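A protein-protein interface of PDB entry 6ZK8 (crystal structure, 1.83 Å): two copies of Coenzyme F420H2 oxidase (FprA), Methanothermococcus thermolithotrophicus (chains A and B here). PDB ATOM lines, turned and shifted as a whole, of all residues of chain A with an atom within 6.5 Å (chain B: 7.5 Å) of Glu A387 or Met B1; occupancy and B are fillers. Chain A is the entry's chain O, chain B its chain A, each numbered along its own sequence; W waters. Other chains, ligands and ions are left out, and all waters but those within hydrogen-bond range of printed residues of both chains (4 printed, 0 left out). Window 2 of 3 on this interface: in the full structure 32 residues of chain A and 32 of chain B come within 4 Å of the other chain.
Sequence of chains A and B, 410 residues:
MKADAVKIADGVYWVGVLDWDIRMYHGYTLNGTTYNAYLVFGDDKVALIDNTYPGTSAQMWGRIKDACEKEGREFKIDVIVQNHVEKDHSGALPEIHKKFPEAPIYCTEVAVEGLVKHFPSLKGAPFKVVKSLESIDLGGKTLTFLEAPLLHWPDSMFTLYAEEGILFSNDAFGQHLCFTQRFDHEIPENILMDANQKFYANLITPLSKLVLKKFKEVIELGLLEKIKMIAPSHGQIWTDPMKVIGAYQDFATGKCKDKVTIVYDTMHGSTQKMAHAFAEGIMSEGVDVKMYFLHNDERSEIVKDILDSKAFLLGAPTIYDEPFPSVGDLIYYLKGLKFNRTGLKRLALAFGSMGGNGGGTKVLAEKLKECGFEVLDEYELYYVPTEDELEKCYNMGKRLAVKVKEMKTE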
ATOM      1  N   LYS A 273       7.721  12.972  10.352  1.00  0.00           N
ATOM      2  CA  LYS A 273       8.097  13.322   8.984  1.00  0.00           C
ATOM      3  C   LYS A 273       7.162  14.374   8.402  1.00  0.00           C
ATOM      4  O   LYS A 273       7.610  15.299   7.716  1.00  0.00           O
ATOM      5  CB  LYS A 273       8.099  12.075   8.108  1.00  0.00           C
ATOM      6  CG  LYS A 273       9.200  11.073   8.454  1.00  0.00           C
ATOM      7  CD  LYS A 273       8.963   9.741   7.755  1.00  0.00           C
ATOM      8  CE  LYS A 273      10.128   8.770   7.937  1.00  0.00           C
ATOM      9  NZ  LYS A 273      10.076   8.062   9.218  1.00  0.00           N
ATOM     10  N   HIS A 276       8.124  17.857   9.961  1.00  0.00           N
ATOM     11  CA  HIS A 276       9.301  18.434   9.310  1.00  0.00           C
ATOM     12  C   HIS A 276       8.999  18.911   7.890  1.00  0.00           C
ATOM     13  O   HIS A 276       9.591  19.897   7.430  1.00  0.00           O
ATOM     14  CB  HIS A 276      10.441  17.426   9.265  1.00  0.00           C
ATOM     15  CG  HIS A 276      10.967  17.050  10.604  1.00  0.00           C
ATOM     16  ND1 HIS A 276      12.066  16.239  10.767  1.00  0.00           N
ATOM     17  CD2 HIS A 276      10.552  17.378  11.849  1.00  0.00           C
ATOM     18  CE1 HIS A 276      12.299  16.073  12.057  1.00  0.00           C
ATOM     19  NE2 HIS A 276      11.373  16.723  12.735  1.00  0.00           N
ATOM     20  N   ALA A 277       8.091  18.227   7.179  1.00  0.00           N
ATOM     21  CA  ALA A 277       7.748  18.629   5.816  1.00  0.00           C
ATOM     22  C   ALA A 277       6.930  19.917   5.803  1.00  0.00           C
ATOM     23  O   ALA A 277       7.129  20.771   4.936  1.00  0.00           O
ATOM     24  CB  ALA A 277       6.996  17.496   5.100  1.00  0.00           C
ATOM     25  N   PHE A 278       5.994  20.067   6.743  1.00  0.00           N
ATOM     26  CA  PHE A 278       5.302  21.343   6.906  1.00  0.00           C
ATOM     27  C   PHE A 278       6.290  22.475   7.158  1.00  0.00           C
ATOM     28  O   PHE A 278       6.116  23.587   6.645  1.00  0.00           O
ATOM     29  CB  PHE A 278       4.313  21.281   8.071  1.00  0.00           C
ATOM     30  CG  PHE A 278       3.033  20.583   7.753  1.00  0.00           C
ATOM     31  CD1 PHE A 278       2.098  21.167   6.939  1.00  0.00           C
ATOM     32  CD2 PHE A 278       2.759  19.337   8.285  1.00  0.00           C
ATOM     33  CE1 PHE A 278       0.928  20.506   6.651  1.00  0.00           C
ATOM     34  CE2 PHE A 278       1.571  18.681   7.983  1.00  0.00           C
ATOM     35  CZ  PHE A 278       0.668  19.272   7.190  1.00  0.00           C
ATOM     36  N   GLU A 280       9.458  22.706   6.186  1.00  0.00           N
ATOM     37  CA  GLU A 280      10.173  23.052   4.966  1.00  0.00           C
ATOM     38  C   GLU A 280       9.345  24.000   4.107  1.00  0.00           C
ATOM     39  O   GLU A 280       9.868  24.984   3.578  1.00  0.00           O
ATOM     40  CB  GLU A 280      10.525  21.790   4.182  1.00  0.00           C
ATOM     41  CG  GLU A 280      11.559  20.877   4.830  1.00  0.00           C
ATOM     42  CD  GLU A 280      12.859  21.585   5.115  1.00  0.00           C
ATOM     43  OE1 GLU A 280      13.216  22.526   4.369  1.00  0.00           O
ATOM     44  OE2 GLU A 280      13.525  21.199   6.096  1.00  0.00           O
ATOM     45  N   PRO A 385       4.368   8.395   5.175  1.00  0.00           N
ATOM     46  CA  PRO A 385       4.134   9.314   4.054  1.00  0.00           C
ATOM     47  C   PRO A 385       4.936   8.920   2.825  1.00  0.00           C
ATOM     48  O   PRO A 385       6.115   8.578   2.916  1.00  0.00           O
ATOM     49  CB  PRO A 385       4.593  10.671   4.597  1.00  0.00           C
ATOM     50  CG  PRO A 385       4.537  10.545   6.052  1.00  0.00           C
ATOM     51  CD  PRO A 385       4.855   9.098   6.374  1.00  0.00           C
ATOM     52  N   THR A 386       4.293   8.996   1.666  1.00  0.00           N
ATOM     53  CA  THR A 386       5.018   8.872   0.402  1.00  0.00           C
ATOM     54  C   THR A 386       5.745  10.181   0.093  1.00  0.00           C
ATOM     55  O   THR A 386       5.579  11.187   0.785  1.00  0.00           O
ATOM     56  CB  THR A 386       4.087   8.535  -0.749  1.00  0.00           C
ATOM     57  OG1 THR A 386       3.180   9.623  -0.930  1.00  0.00           O
ATOM     58  CG2 THR A 386       3.327   7.234  -0.489  1.00  0.00           C
ATOM     59  N   GLU A 387       6.566  10.157  -0.959  1.00  0.00           N
ATOM     60  CA  GLU A 387       7.217  11.378  -1.425  1.00  0.00           C
ATOM     61  C   GLU A 387       6.186  12.452  -1.754  1.00  0.00           C
ATOM     62  O   GLU A 387       6.327  13.612  -1.348  1.00  0.00           O
ATOM     63  CB  GLU A 387       8.072  11.067  -2.658  1.00  0.00           C
ATOM     64  CG  GLU A 387       9.407  11.777  -2.681  1.00  0.00           C
ATOM     65  CD  GLU A 387      10.426  11.112  -1.775  1.00  0.00           C
ATOM     66  OE1 GLU A 387      10.590   9.878  -1.906  1.00  0.00           O
ATOM     67  OE2 GLU A 387      11.037  11.813  -0.925  1.00  0.00           O
ATOM     68  N   ASP A 388       5.131  12.078  -2.485  1.00  0.00           N
ATOM     69  CA  ASP A 388       4.115  13.050  -2.865  1.00  0.00           C
ATOM     70  C   ASP A 388       3.383  13.602  -1.651  1.00  0.00           C
ATOM     71  O   ASP A 388       2.987  14.772  -1.637  1.00  0.00           O
ATOM     72  CB  ASP A 388       3.108  12.409  -3.821  1.00  0.00           C
ATOM     73  CG  ASP A 388       3.698  12.118  -5.179  1.00  0.00           C
ATOM     74  OD1 ASP A 388       4.669  12.797  -5.575  1.00  0.00           O
ATOM     75  OD2 ASP A 388       3.180  11.219  -5.863  1.00  0.00           O
ATOM     76  N   GLU A 389       3.153  12.769  -0.641  1.00  0.00           N
ATOM     77  CA  GLU A 389       2.419  13.223   0.528  1.00  0.00           C
ATOM     78  C   GLU A 389       3.233  14.208   1.349  1.00  0.00           C
ATOM     79  O   GLU A 389       2.671  15.150   1.912  1.00  0.00           O
ATOM     80  CB  GLU A 389       2.003  12.012   1.367  1.00  0.00           C
ATOM     81  CG  GLU A 389       0.921  11.189   0.697  1.00  0.00           C
ATOM     82  CD  GLU A 389       0.536   9.955   1.477  1.00  0.00           C
ATOM     83  OE1 GLU A 389       1.445   9.306   2.035  1.00  0.00           O
ATOM     84  OE2 GLU A 389      -0.675   9.642   1.525  1.00  0.00           O
ATOM     85  N   LEU A 390       4.551  14.023   1.421  1.00  0.00           N
ATOM     86  CA  LEU A 390       5.389  15.029   2.052  1.00  0.00           C
ATOM     87  C   LEU A 390       5.392  16.315   1.235  1.00  0.00           C
ATOM     88  O   LEU A 390       5.466  17.407   1.804  1.00  0.00           O
ATOM     89  CB  LEU A 390       6.816  14.497   2.222  1.00  0.00           C
ATOM     90  CG  LEU A 390       6.994  13.309   3.165  1.00  0.00           C
ATOM     91  CD1 LEU A 390       8.412  12.755   3.068  1.00  0.00           C
ATOM     92  CD2 LEU A 390       6.668  13.674   4.629  1.00  0.00           C
ATOM     93  N   GLU A 391       5.281  16.214  -0.091  1.00  0.00           N
ATOM     94  CA  GLU A 391       5.188  17.421  -0.899  1.00  0.00           C
ATOM     95  C   GLU A 391       3.880  18.156  -0.648  1.00  0.00           C
ATOM     96  O   GLU A 391       3.848  19.393  -0.702  1.00  0.00           O
ATOM     97  CB  GLU A 391       5.325  17.086  -2.380  1.00  0.00           C
ATOM     98  CG  GLU A 391       5.367  18.328  -3.277  1.00  0.00           C
ATOM     99  CD  GLU A 391       5.830  18.026  -4.686  1.00  0.00           C
ATOM    100  OE1 GLU A 391       5.847  16.834  -5.080  1.00  0.00           O
ATOM    101  OE2 GLU A 391       6.172  18.993  -5.409  1.00  0.00           O
ATOM    102  N   LYS A 392       2.799  17.419  -0.367  1.00  0.00           N
ATOM    103  CA  LYS A 392       1.550  18.070   0.011  1.00  0.00           C
ATOM    104  C   LYS A 392       1.700  18.808   1.336  1.00  0.00           C
ATOM    105  O   LYS A 392       1.208  19.938   1.476  1.00  0.00           O
ATOM    106  CB  LYS A 392       0.421  17.049   0.094  1.00  0.00           C
ATOM    107  CG  LYS A 392      -0.880  17.602   0.653  1.00  0.00           C
ATOM    108  CD  LYS A 392      -2.088  16.742   0.212  1.00  0.00           C
ATOM    109  CE  LYS A 392      -3.367  17.203   0.908  1.00  0.00           C
ATOM    110  NZ  LYS A 392      -3.788  18.586   0.479  1.00  0.00           N
ATOM    111  N   MET B   1      11.868  13.869   0.082  1.00  0.00           N
ATOM    112  CA  MET B   1      11.340  15.073   0.795  1.00  0.00           C
ATOM    113  C   MET B   1      11.757  16.361   0.100  1.00  0.00           C
ATOM    114  O   MET B   1      12.908  16.499  -0.327  1.00  0.00           O
ATOM    115  CB  MET B   1      11.853  15.046   2.216  1.00  0.00           C
ATOM    116  CG  MET B   1      11.426  16.213   3.079  1.00  0.00           C
ATOM    117  SD  MET B   1      12.013  15.935   4.724  1.00  0.00           S
ATOM    118  CE  MET B   1      11.458  17.436   5.552  1.00  0.00           C
ATOM    119  N   LYS B   2      10.821  17.304  -0.019  1.00  0.00           N
ATOM    120  CA  LYS B   2      11.121  18.591  -0.618  1.00  0.00           C
ATOM    121  C   LYS B   2      11.674  19.514   0.464  1.00  0.00           C
ATOM    122  O   LYS B   2      11.056  19.693   1.520  1.00  0.00           O
ATOM    123  CB  LYS B   2       9.886  19.194  -1.288  1.00  0.00           C
ATOM    124  CG  LYS B   2      10.247  20.340  -2.194  1.00  0.00           C
ATOM    125  CD  LYS B   2       9.048  20.927  -2.934  1.00  0.00           C
ATOM    126  CE  LYS B   2       9.487  22.064  -3.844  1.00  0.00           C
ATOM    127  NZ  LYS B   2       8.323  22.757  -4.509  1.00  0.00           N
ATOM    128  N   ALA B   3      12.840  20.096   0.188  1.00  0.00           N
ATOM    129  CA  ALA B   3      13.535  20.966   1.121  1.00  0.00           C
ATOM    130  C   ALA B   3      14.438  21.900   0.331  1.00  0.00           C
ATOM    131  O   ALA B   3      15.185  21.452  -0.535  1.00  0.00           O
ATOM    132  CB  ALA B   3      14.347  20.144   2.123  1.00  0.00           C
ATOM    133  N   ASP B   4      14.383  23.187   0.639  1.00  0.00           N
ATOM    134  CA  ASP B   4      15.106  24.191  -0.133  1.00  0.00           C
ATOM    135  C   ASP B   4      16.536  24.364   0.356  1.00  0.00           C
ATOM    136  O   ASP B   4      16.794  24.415   1.556  1.00  0.00           O
ATOM    137  CB  ASP B   4      14.389  25.543  -0.046  1.00  0.00           C
ATOM    138  CG  ASP B   4      12.984  25.513  -0.617  1.00  0.00           C
ATOM    139  OD1 ASP B   4      12.441  24.415  -0.871  1.00  0.00           O
ATOM    140  OD2 ASP B   4      12.423  26.611  -0.815  1.00  0.00           O
ATOM    141  N   TRP B  20      15.840  18.899  14.390  1.00  0.00           N
ATOM    142  CA  TRP B  20      15.006  19.649  15.317  1.00  0.00           C
ATOM    143  C   TRP B  20      14.947  19.003  16.688  1.00  0.00           C
ATOM    144  O   TRP B  20      14.906  19.708  17.698  1.00  0.00           O
ATOM    145  CB  TRP B  20      13.587  19.769  14.778  1.00  0.00           C
ATOM    146  CG  TRP B  20      13.437  20.384  13.437  1.00  0.00           C
ATOM    147  CD1 TRP B  20      13.287  19.724  12.251  1.00  0.00           C
ATOM    148  CD2 TRP B  20      13.358  21.781  13.131  1.00  0.00           C
ATOM    149  NE1 TRP B  20      13.115  20.629  11.223  1.00  0.00           N
ATOM    150  CE2 TRP B  20      13.164  21.894  11.737  1.00  0.00           C
ATOM    151  CE3 TRP B  20      13.433  22.941  13.894  1.00  0.00           C
ATOM    152  CZ2 TRP B  20      13.057  23.107  11.102  1.00  0.00           C
ATOM    153  CZ3 TRP B  20      13.324  24.149  13.258  1.00  0.00           C
ATOM    154  CH2 TRP B  20      13.127  24.222  11.870  1.00  0.00           C
ATOM    155  N   SER B  57      19.162  11.668   5.813  1.00  0.00           N
ATOM    156  CA  SER B  57      19.568  12.234   4.525  1.00  0.00           C
ATOM    157  C   SER B  57      18.420  12.826   3.708  1.00  0.00           C
ATOM    158  O   SER B  57      18.687  13.547   2.739  1.00  0.00           O
ATOM    159  CB  SER B  57      20.274  11.185   3.677  1.00  0.00           C
ATOM    160  OG  SER B  57      19.365  10.193   3.211  1.00  0.00           O
ATOM    161  N   ALA B  58      17.165  12.583   4.085  1.00  0.00           N
ATOM    162  CA  ALA B  58      16.044  13.040   3.270  1.00  0.00           C
ATOM    163  C   ALA B  58      16.092  14.552   3.035  1.00  0.00           C
ATOM    164  O   ALA B  58      15.901  15.023   1.910  1.00  0.00           O
ATOM    165  CB  ALA B  58      14.726  12.631   3.926  1.00  0.00           C
ATOM    166  N   GLN B  59      16.346  15.333   4.084  1.00  0.00           N
ATOM    167  CA  GLN B  59      16.482  16.776   3.915  1.00  0.00           C
ATOM    168  C   GLN B  59      17.650  17.114   2.994  1.00  0.00           C
ATOM    169  O   GLN B  59      17.538  17.982   2.109  1.00  0.00           O
ATOM    170  CB  GLN B  59      16.682  17.447   5.276  1.00  0.00           C
ATOM    171  CG  GLN B  59      15.443  17.661   6.105  1.00  0.00           C
ATOM    172  CD  GLN B  59      15.768  18.347   7.406  1.00  0.00           C
ATOM    173  OE1 GLN B  59      16.580  19.278   7.435  1.00  0.00           O
ATOM    174  NE2 GLN B  59      15.163  17.891   8.495  1.00  0.00           N
ATOM    175  N   MET B  60      18.796  16.465   3.215  1.00  0.00           N
ATOM    176  CA  MET B  60      19.984  16.767   2.424  1.00  0.00           C
ATOM    177  C   MET B  60      19.715  16.569   0.939  1.00  0.00           C
ATOM    178  O   MET B  60      20.010  17.444   0.123  1.00  0.00           O
ATOM    179  CB  MET B  60      21.153  15.893   2.880  1.00  0.00           C
ATOM    180  CG  MET B  60      22.483  16.224   2.232  1.00  0.00           C
ATOM    181  SD  MET B  60      23.729  14.947   2.551  1.00  0.00           S
ATOM    182  CE  MET B  60      23.159  13.607   1.499  1.00  0.00           C
ATOM    183  N   TRP B  61      19.157  15.421   0.567  1.00  0.00           N
ATOM    184  CA  TRP B  61      18.922  15.147  -0.844  1.00  0.00           C
ATOM    185  C   TRP B  61      17.925  16.129  -1.433  1.00  0.00           C
ATOM    186  O   TRP B  61      18.040  16.528  -2.597  1.00  0.00           O
ATOM    187  CB  TRP B  61      18.434  13.717  -1.028  1.00  0.00           C
ATOM    188  CG  TRP B  61      19.512  12.687  -0.849  1.00  0.00           C
ATOM    189  CD1 TRP B  61      19.535  11.699   0.065  1.00  0.00           C
ATOM    190  CD2 TRP B  61      20.723  12.555  -1.609  1.00  0.00           C
ATOM    191  NE1 TRP B  61      20.665  10.940  -0.084  1.00  0.00           N
ATOM    192  CE2 TRP B  61      21.420  11.457  -1.096  1.00  0.00           C
ATOM    193  CE3 TRP B  61      21.275  13.259  -2.673  1.00  0.00           C
ATOM    194  CZ2 TRP B  61      22.643  11.043  -1.604  1.00  0.00           C
ATOM    195  CZ3 TRP B  61      22.489  12.866  -3.161  1.00  0.00           C
ATOM    196  CH2 TRP B  61      23.158  11.757  -2.636  1.00  0.00           C
ATOM    197  N   GLY B  62      16.934  16.530  -0.649  1.00  0.00           N
ATOM    198  CA  GLY B  62      15.995  17.523  -1.138  1.00  0.00           C
ATOM    199  C   GLY B  62      16.669  18.842  -1.446  1.00  0.00           C
ATOM    200  O   GLY B  62      16.379  19.480  -2.460  1.00  0.00           O
ATOM    201  N   ARG B  63      17.579  19.269  -0.571  1.00  0.00           N
ATOM    202  CA  ARG B  63      18.263  20.540  -0.778  1.00  0.00           C
ATOM    203  C   ARG B  63      19.269  20.429  -1.913  1.00  0.00           C
ATOM    204  O   ARG B  63      19.469  21.383  -2.662  1.00  0.00           O
ATOM    205  CB  ARG B  63      18.942  21.004   0.516  1.00  0.00           C
ATOM    206  CG  ARG B  63      17.985  21.212   1.689  1.00  0.00           C
ATOM    207  CD  ARG B  63      18.659  21.845   2.901  1.00  0.00           C
ATOM    208  NE  ARG B  63      18.026  21.413   4.158  1.00  0.00           N
ATOM    209  CZ  ARG B  63      16.844  21.846   4.590  1.00  0.00           C
ATOM    210  NH1 ARG B  63      16.154  22.731   3.874  1.00  0.00           N
ATOM    211  NH2 ARG B  63      16.352  21.404   5.747  1.00  0.00           N
ATOM    212  N   LYS B  65      18.926  18.497  -4.575  1.00  0.00           N
ATOM    213  CA  LYS B  65      18.091  18.589  -5.760  1.00  0.00           C
ATOM    214  C   LYS B  65      17.675  20.024  -6.028  1.00  0.00           C
ATOM    215  O   LYS B  65      17.708  20.479  -7.173  1.00  0.00           O
ATOM    216  CB  LYS B  65      16.869  17.693  -5.595  1.00  0.00           C
ATOM    217  CG  LYS B  65      17.157  16.215  -5.807  1.00  0.00           C
ATOM    218  CD  LYS B  65      15.881  15.382  -5.678  1.00  0.00           C
ATOM    219  CE  LYS B  65      16.141  13.907  -6.001  1.00  0.00           C
ATOM    220  NZ  LYS B  65      14.937  13.053  -5.733  1.00  0.00           N
HETATM  221  O   HOH W   1      12.169  20.404   8.488  1.00  0.00           O
HETATM  222  O   HOH W   2      13.533  15.508   8.538  1.00  0.00           O
HETATM  223  O   HOH W   3      12.419  24.526   2.921  1.00  0.00           O
HETATM  224  O   HOH W   4       8.745  17.890   1.835  1.00  0.00           O
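No position is printed for both chains.
Of chain B, only Met B1 comes within 4 Å of Glu A387.
Met B1 touches four residues of chain A.
Of the printed residues of chain B, Ala A277 touches Met B1 (3.8 Å).
Of the printed residues of chain A, Trp B20 touches His A276.
Of the printed residues of chain B, His A276 touches Met B1 and Trp B20.
The nearest residue of chain A that does not touch Met B1 is Leu A390 (4.2 Å).
The nearest printed residue of chain B that does not touch Glu A280 is Trp B20 (5.2 Å).
O of Ala B3 sits close to N of Arg B63 (3.2 Å).
OE1 of Gln B59 sits at hydrogen-bond distance from NH2 of Arg B63, 2.7 Å away.
The guanidinium group (NH1) of Arg B63 sits at hydrogen-bond distance from the backbone carbonyl oxygen (O) of Asp B4.
N of Met B1 is in hydrogen-bond range of OE2 of Glu A387 (2.4 Å).
The side-chain carboxylate of Glu A280 lies within salt-bridge range of the guanidinium group of Arg B63 (2.9 Å).
Of the 13 printed residues of chain B, 7 touch a printed residue of chain A.
Hydrophobic or aromatic side chains of chain B that line the printed part of chain A: Met B1, Ala B3 and Trp B20.
Printed residues of chain A that touch a printed residue of chain B: His A276, Ala A277, Glu A280 and Glu A387.
Hydrophobic or aromatic side chains of chain A that line the printed part of chain B: His A276.
Among the printed residues, 10 pairs touch across the chains.
Among the printed residues, Asp or Glu carboxylates within 4 Å of a Lys or Arg side-chain nitrogen of the other chain: Glu A280 with Arg B63 (2.9 Å).
Water W3 lies within hydrogen-bond range of the side-chain carboxylate of Glu A280 (2.6 Å) and the backbone NH of Asp B4 (3.3 Å).
Water W2 lies within hydrogen-bond range of a ring nitrogen (ND1) of His A276 (2.8 Å) and the side-chain amide nitrogen (NE2) of Gln B59 (2.9 Å).
Water W1 lies within hydrogen-bond range of O of His A276 (2.8 Å), OE2 of Glu A280 (2.9 Å) and NE1 of Trp B20 (2.9 Å).
Water W4 lies within hydrogen-bond range of the backbone NH (N) of Lys B2 (2.8 Å) and the backbone carbonyl oxygen (O) of Leu A390 (3.3 Å).
Among the printed residues, merely in contact across the chains: Glu A280 with Lys B2 (3.4 Å), Glu A280 with Ala B3 (3.5 Å), Glu A280 with Met B1 (3.5 Å), His A276 with Trp B20 (3.6 Å), His A276 with Met B1 (3.6 Å), Ala A277 with Met B1 (3.8 Å), Glu A280 with Gln B59 (3.8 Å) and Glu A280 with Asp B4 (3.96 Å).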
